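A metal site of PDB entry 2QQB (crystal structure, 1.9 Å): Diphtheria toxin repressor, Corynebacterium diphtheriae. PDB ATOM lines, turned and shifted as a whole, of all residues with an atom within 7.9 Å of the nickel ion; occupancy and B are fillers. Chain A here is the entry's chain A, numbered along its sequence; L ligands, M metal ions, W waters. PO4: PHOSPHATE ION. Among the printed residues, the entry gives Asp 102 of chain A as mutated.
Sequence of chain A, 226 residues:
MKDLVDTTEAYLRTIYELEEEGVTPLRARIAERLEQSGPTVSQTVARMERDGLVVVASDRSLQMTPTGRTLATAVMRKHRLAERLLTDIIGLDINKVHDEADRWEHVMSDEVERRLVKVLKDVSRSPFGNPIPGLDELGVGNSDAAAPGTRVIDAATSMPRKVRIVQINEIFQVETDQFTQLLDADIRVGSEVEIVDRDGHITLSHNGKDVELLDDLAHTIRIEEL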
ATOM      1  N   ARG A  13     -17.714   3.127   4.536  1.00  0.00           N
ATOM      2  CA  ARG A  13     -17.148   4.436   4.920  1.00  0.00           C
ATOM      3  C   ARG A  13     -17.112   4.562   6.494  1.00  0.00           C
ATOM      4  O   ARG A  13     -16.171   5.138   7.046  1.00  0.00           O
ATOM      5  CB  ARG A  13     -17.967   5.565   4.253  1.00  0.00           C
ATOM      6  CG  ARG A  13     -17.202   6.836   3.895  1.00  0.00           C
ATOM      7  CD  ARG A  13     -17.400   8.005   4.893  1.00  0.00           C
ATOM      8  NE  ARG A  13     -18.732   8.643   4.655  1.00  0.00           N
ATOM      9  CZ  ARG A  13     -19.537   9.108   5.588  1.00  0.00           C
ATOM     10  NH1 ARG A  13     -19.137   9.095   6.846  1.00  0.00           N
ATOM     11  NH2 ARG A  13     -20.744   9.626   5.274  1.00  0.00           N
ATOM     12  N   GLU A  17     -13.692   5.066   8.681  1.00  0.00           N
ATOM     13  CA  GLU A  17     -13.560   6.193   9.570  1.00  0.00           C
ATOM     14  C   GLU A  17     -13.235   5.813  11.046  1.00  0.00           C
ATOM     15  O   GLU A  17     -12.369   6.432  11.633  1.00  0.00           O
ATOM     16  CB  GLU A  17     -14.681   7.226   9.389  1.00  0.00           C
ATOM     17  CG  GLU A  17     -16.083   6.803   9.784  1.00  0.00           C
ATOM     18  CD  GLU A  17     -17.155   7.906   9.561  1.00  0.00           C
ATOM     19  OE1 GLU A  17     -18.159   7.759  10.260  1.00  0.00           O
ATOM     20  OE2 GLU A  17     -16.959   8.884   8.730  1.00  0.00           O
ATOM     21  N   MET A  76     -15.022   7.122   0.502  1.00  0.00           N
ATOM     22  CA  MET A  76     -14.414   8.155   1.269  1.00  0.00           C
ATOM     23  C   MET A  76     -13.820   9.349   0.492  1.00  0.00           C
ATOM     24  O   MET A  76     -13.926  10.507   0.958  1.00  0.00           O
ATOM     25  CB  MET A  76     -13.337   7.628   2.226  1.00  0.00           C
ATOM     26  CG  MET A  76     -12.767   8.713   3.160  1.00  0.00           C
ATOM     27  SD  MET A  76     -13.968   9.501   4.334  1.00  0.00           S
ATOM     28  CE  MET A  76     -13.677   8.444   5.758  1.00  0.00           C
ATOM     29  N   HIS A  79     -16.625  11.414  -0.814  1.00  0.00           N
ATOM     30  CA  HIS A  79     -17.237  12.112   0.281  1.00  0.00           C
ATOM     31  C   HIS A  79     -16.439  13.361   0.535  1.00  0.00           C
ATOM     32  O   HIS A  79     -16.964  14.438   0.523  1.00  0.00           O
ATOM     33  CB  HIS A  79     -17.320  11.230   1.532  1.00  0.00           C
ATOM     34  CG  HIS A  79     -17.876  11.943   2.684  1.00  0.00           C
ATOM     35  ND1 HIS A  79     -19.207  12.206   2.807  1.00  0.00           N
ATOM     36  CD2 HIS A  79     -17.260  12.520   3.772  1.00  0.00           C
ATOM     37  CE1 HIS A  79     -19.413  12.899   3.907  1.00  0.00           C
ATOM     38  NE2 HIS A  79     -18.254  13.075   4.516  1.00  0.00           N
ATOM     39  N   ARG A  80     -15.127  13.196   0.671  1.00  0.00           N
ATOM     40  CA  ARG A  80     -14.256  14.290   0.965  1.00  0.00           C
ATOM     41  C   ARG A  80     -14.170  15.390  -0.143  1.00  0.00           C
ATOM     42  O   ARG A  80     -14.215  16.548   0.154  1.00  0.00           O
ATOM     43  CB  ARG A  80     -12.883  13.784   1.473  1.00  0.00           C
ATOM     44  CG  ARG A  80     -13.018  13.240   2.917  1.00  0.00           C
ATOM     45  CD  ARG A  80     -11.816  12.534   3.464  1.00  0.00           C
ATOM     46  NE  ARG A  80     -12.265  12.121   4.768  1.00  0.00           N
ATOM     47  CZ  ARG A  80     -11.672  11.308   5.655  1.00  0.00           C
ATOM     48  NH1 ARG A  80     -10.487  10.783   5.433  1.00  0.00           N
ATOM     49  NH2 ARG A  80     -12.369  10.997   6.784  1.00  0.00           N
ATOM     50  N   GLU A  83     -17.382  17.403  -0.149  1.00  0.00           N
ATOM     51  CA  GLU A  83     -17.193  18.405   0.890  1.00  0.00           C
ATOM     52  C   GLU A  83     -16.378  19.660   0.474  1.00  0.00           C
ATOM     53  O   GLU A  83     -16.859  20.759   0.732  1.00  0.00           O
ATOM     54  CB  GLU A  83     -16.620  17.716   2.140  1.00  0.00           C
ATOM     55  CG  GLU A  83     -17.748  16.793   2.779  1.00  0.00           C
ATOM     56  CD  GLU A  83     -17.243  16.150   4.092  1.00  0.00           C
ATOM     57  OE1 GLU A  83     -16.023  15.911   4.254  1.00  0.00           O
ATOM     58  OE2 GLU A  83     -18.116  15.922   4.940  1.00  0.00           O
ATOM     59  N   VAL A  97     -22.511  21.045   5.169  1.00  0.00           N
ATOM     60  CA  VAL A  97     -21.616  20.437   4.138  1.00  0.00           C
ATOM     61  C   VAL A  97     -21.481  18.941   4.247  1.00  0.00           C
ATOM     62  O   VAL A  97     -21.587  18.250   3.192  1.00  0.00           O
ATOM     63  CB  VAL A  97     -20.255  21.107   4.012  1.00  0.00           C
ATOM     64  CG1 VAL A  97     -19.226  20.125   3.288  1.00  0.00           C
ATOM     65  CG2 VAL A  97     -20.341  22.493   3.262  1.00  0.00           C
ATOM     66  N   HIS A  98     -21.274  18.433   5.489  1.00  0.00           N
ATOM     67  CA  HIS A  98     -21.157  17.002   5.748  1.00  0.00           C
ATOM     68  C   HIS A  98     -22.410  16.227   5.336  1.00  0.00           C
ATOM     69  O   HIS A  98     -22.323  15.169   4.709  1.00  0.00           O
ATOM     70  CB  HIS A  98     -20.668  16.609   7.193  1.00  0.00           C
ATOM     71  CG  HIS A  98     -20.937  15.145   7.522  1.00  0.00           C
ATOM     72  ND1 HIS A  98     -20.161  14.111   7.050  1.00  0.00           N
ATOM     73  CD2 HIS A  98     -21.978  14.563   8.138  1.00  0.00           C
ATOM     74  CE1 HIS A  98     -20.666  12.964   7.455  1.00  0.00           C
ATOM     75  NE2 HIS A  98     -21.825  13.203   8.003  1.00  0.00           N
ATOM     76  N   ASP A  99     -23.595  16.725   5.790  1.00  0.00           N
ATOM     77  CA  ASP A  99     -24.815  15.955   5.637  1.00  0.00           C
ATOM     78  C   ASP A  99     -25.137  15.782   4.114  1.00  0.00           C
ATOM     79  O   ASP A  99     -25.677  14.752   3.594  1.00  0.00           O
ATOM     80  CB  ASP A  99     -25.950  16.706   6.383  1.00  0.00           C
ATOM     81  CG  ASP A  99     -25.908  16.471   7.897  1.00  0.00           C
ATOM     82  OD1 ASP A  99     -25.276  15.478   8.346  1.00  0.00           O
ATOM     83  OD2 ASP A  99     -26.556  17.265   8.640  1.00  0.00           O
ATOM     84  N   ALA A 101     -22.731  16.026   1.578  1.00  0.00           N
ATOM     85  CA  ALA A 101     -21.634  15.056   1.107  1.00  0.00           C
ATOM     86  C   ALA A 101     -21.973  13.577   1.466  1.00  0.00           C
ATOM     87  O   ALA A 101     -21.562  12.673   0.762  1.00  0.00           O
ATOM     88  CB  ALA A 101     -20.288  15.410   1.659  1.00  0.00           C
ATOM     89  N   ASP A 102     -22.789  13.389   2.508  1.00  0.00           N
ATOM     90  CA  ASP A 102     -23.269  12.052   2.943  1.00  0.00           C
ATOM     91  C   ASP A 102     -24.270  11.495   1.850  1.00  0.00           C
ATOM     92  O   ASP A 102     -24.505  10.326   1.708  1.00  0.00           O
ATOM     93  CB  ASP A 102     -23.934  12.206   4.373  1.00  0.00           C
ATOM     94  CG  ASP A 102     -24.037  10.860   5.184  1.00  0.00           C
ATOM     95  OD1 ASP A 102     -23.531   9.832   4.740  1.00  0.00           O
ATOM     96  OD2 ASP A 102     -24.636  10.862   6.331  1.00  0.00           O
ATOM     97  N   GLU A 105     -21.693  11.404  -1.742  1.00  0.00           N
ATOM     98  CA  GLU A 105     -20.697  10.308  -1.801  1.00  0.00           C
ATOM     99  C   GLU A 105     -21.139   9.028  -2.580  1.00  0.00           C
ATOM    100  O   GLU A 105     -20.298   8.319  -3.193  1.00  0.00           O
ATOM    101  CB  GLU A 105     -20.298   9.885  -0.429  1.00  0.00           C
ATOM    102  CG  GLU A 105     -21.347   9.200   0.385  1.00  0.00           C
ATOM    103  CD  GLU A 105     -20.673   9.010   1.738  1.00  0.00           C
ATOM    104  OE1 GLU A 105     -19.409   8.958   1.759  1.00  0.00           O
ATOM    105  OE2 GLU A 105     -21.355   9.031   2.708  1.00  0.00           O
ATOM    106  N   SER A 126      -9.969  17.059   3.326  1.00  0.00           N
ATOM    107  CA  SER A 126     -11.351  17.478   3.449  1.00  0.00           C
ATOM    108  C   SER A 126     -11.427  18.821   4.264  1.00  0.00           C
ATOM    109  O   SER A 126     -10.466  19.195   4.880  1.00  0.00           O
ATOM    110  CB  SER A 126     -12.116  16.336   4.112  1.00  0.00           C
ATOM    111  OG  SER A 126     -12.178  16.409   5.487  1.00  0.00           O
ATOM    112  N   PRO A 127     -12.565  19.546   4.224  1.00  0.00           N
ATOM    113  CA  PRO A 127     -12.643  20.766   5.023  1.00  0.00           C
ATOM    114  C   PRO A 127     -12.613  20.427   6.510  1.00  0.00           C
ATOM    115  O   PRO A 127     -12.451  21.306   7.354  1.00  0.00           O
ATOM    116  CB  PRO A 127     -14.059  21.301   4.695  1.00  0.00           C
ATOM    117  CG  PRO A 127     -14.443  20.656   3.471  1.00  0.00           C
ATOM    118  CD  PRO A 127     -13.845  19.292   3.572  1.00  0.00           C
ATOM    119  N   PHE A 128     -12.845  19.163   6.836  1.00  0.00           N
ATOM    120  CA  PHE A 128     -12.834  18.715   8.232  1.00  0.00           C
ATOM    121  C   PHE A 128     -11.474  18.122   8.723  1.00  0.00           C
ATOM    122  O   PHE A 128     -11.396  17.592   9.806  1.00  0.00           O
ATOM    123  CB  PHE A 128     -14.076  17.806   8.502  1.00  0.00           C
ATOM    124  CG  PHE A 128     -15.322  18.385   7.940  1.00  0.00           C
ATOM    125  CD1 PHE A 128     -16.015  19.401   8.641  1.00  0.00           C
ATOM    126  CD2 PHE A 128     -15.763  18.029   6.697  1.00  0.00           C
ATOM    127  CE1 PHE A 128     -17.117  19.969   8.094  1.00  0.00           C
ATOM    128  CE2 PHE A 128     -16.903  18.615   6.173  1.00  0.00           C
ATOM    129  CZ  PHE A 128     -17.555  19.572   6.805  1.00  0.00           C
ATOM    130  N   ASN A 130      -9.161  15.895   7.330  1.00  0.00           N
ATOM    131  CA  ASN A 130      -8.806  14.514   7.215  1.00  0.00           C
ATOM    132  C   ASN A 130      -8.209  14.346   5.833  1.00  0.00           C
ATOM    133  O   ASN A 130      -8.737  14.919   4.860  1.00  0.00           O
ATOM    134  CB  ASN A 130     -10.075  13.709   7.352  1.00  0.00           C
ATOM    135  CG  ASN A 130     -10.588  13.615   8.788  1.00  0.00           C
ATOM    136  OD1 ASN A 130      -9.835  13.265   9.697  1.00  0.00           O
ATOM    137  ND2 ASN A 130     -11.870  13.810   8.963  1.00  0.00           N
HETATM  138  P   PO4 L   1     -14.661  13.990   7.188  1.00  0.00           P
HETATM  139  O1  PO4 L   1     -13.327  14.347   6.632  1.00  0.00           O
HETATM  140  O2  PO4 L   1     -15.739  14.064   6.073  1.00  0.00           O
HETATM  141  O3  PO4 L   1     -15.103  14.713   8.355  1.00  0.00           O
HETATM  142  O4  PO4 L   1     -14.626  12.518   7.390  1.00  0.00           O
HETATM  143 NI    NI M   1     -17.935  14.099   6.275  1.00  0.00          NI
HETATM  144  O   HOH W   1     -17.417  12.239   7.530  1.00  0.00           O
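The backbone carbonyl oxygen of Ala 101 lies within hydrogen-bond range of a ring nitrogen (ND1) of His 79.
The side-chain carboxylate (OE1) of Glu 105 sits close to a ring nitrogen (ND1) of His 79 (3.4 Å).
NE2 of His 79 is bound to the nickel ion, 2.1 Å away.
O2 of the ligand is bound to the nickel ion, at 2.2 Å.
The side-chain carboxylate (OE2) of Glu 83 is bound to the nickel ion, at 2.3 Å.
Water W1 is bound to the nickel ion, at 2.3 Å.
A ring nitrogen (ND1) of His 98 is bound to the nickel ion (2.4 Å).
The nickel ion has five donor atoms within binding distance.
Within 4 Å of the nickel ion: His 79, Glu 83 and His 98.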
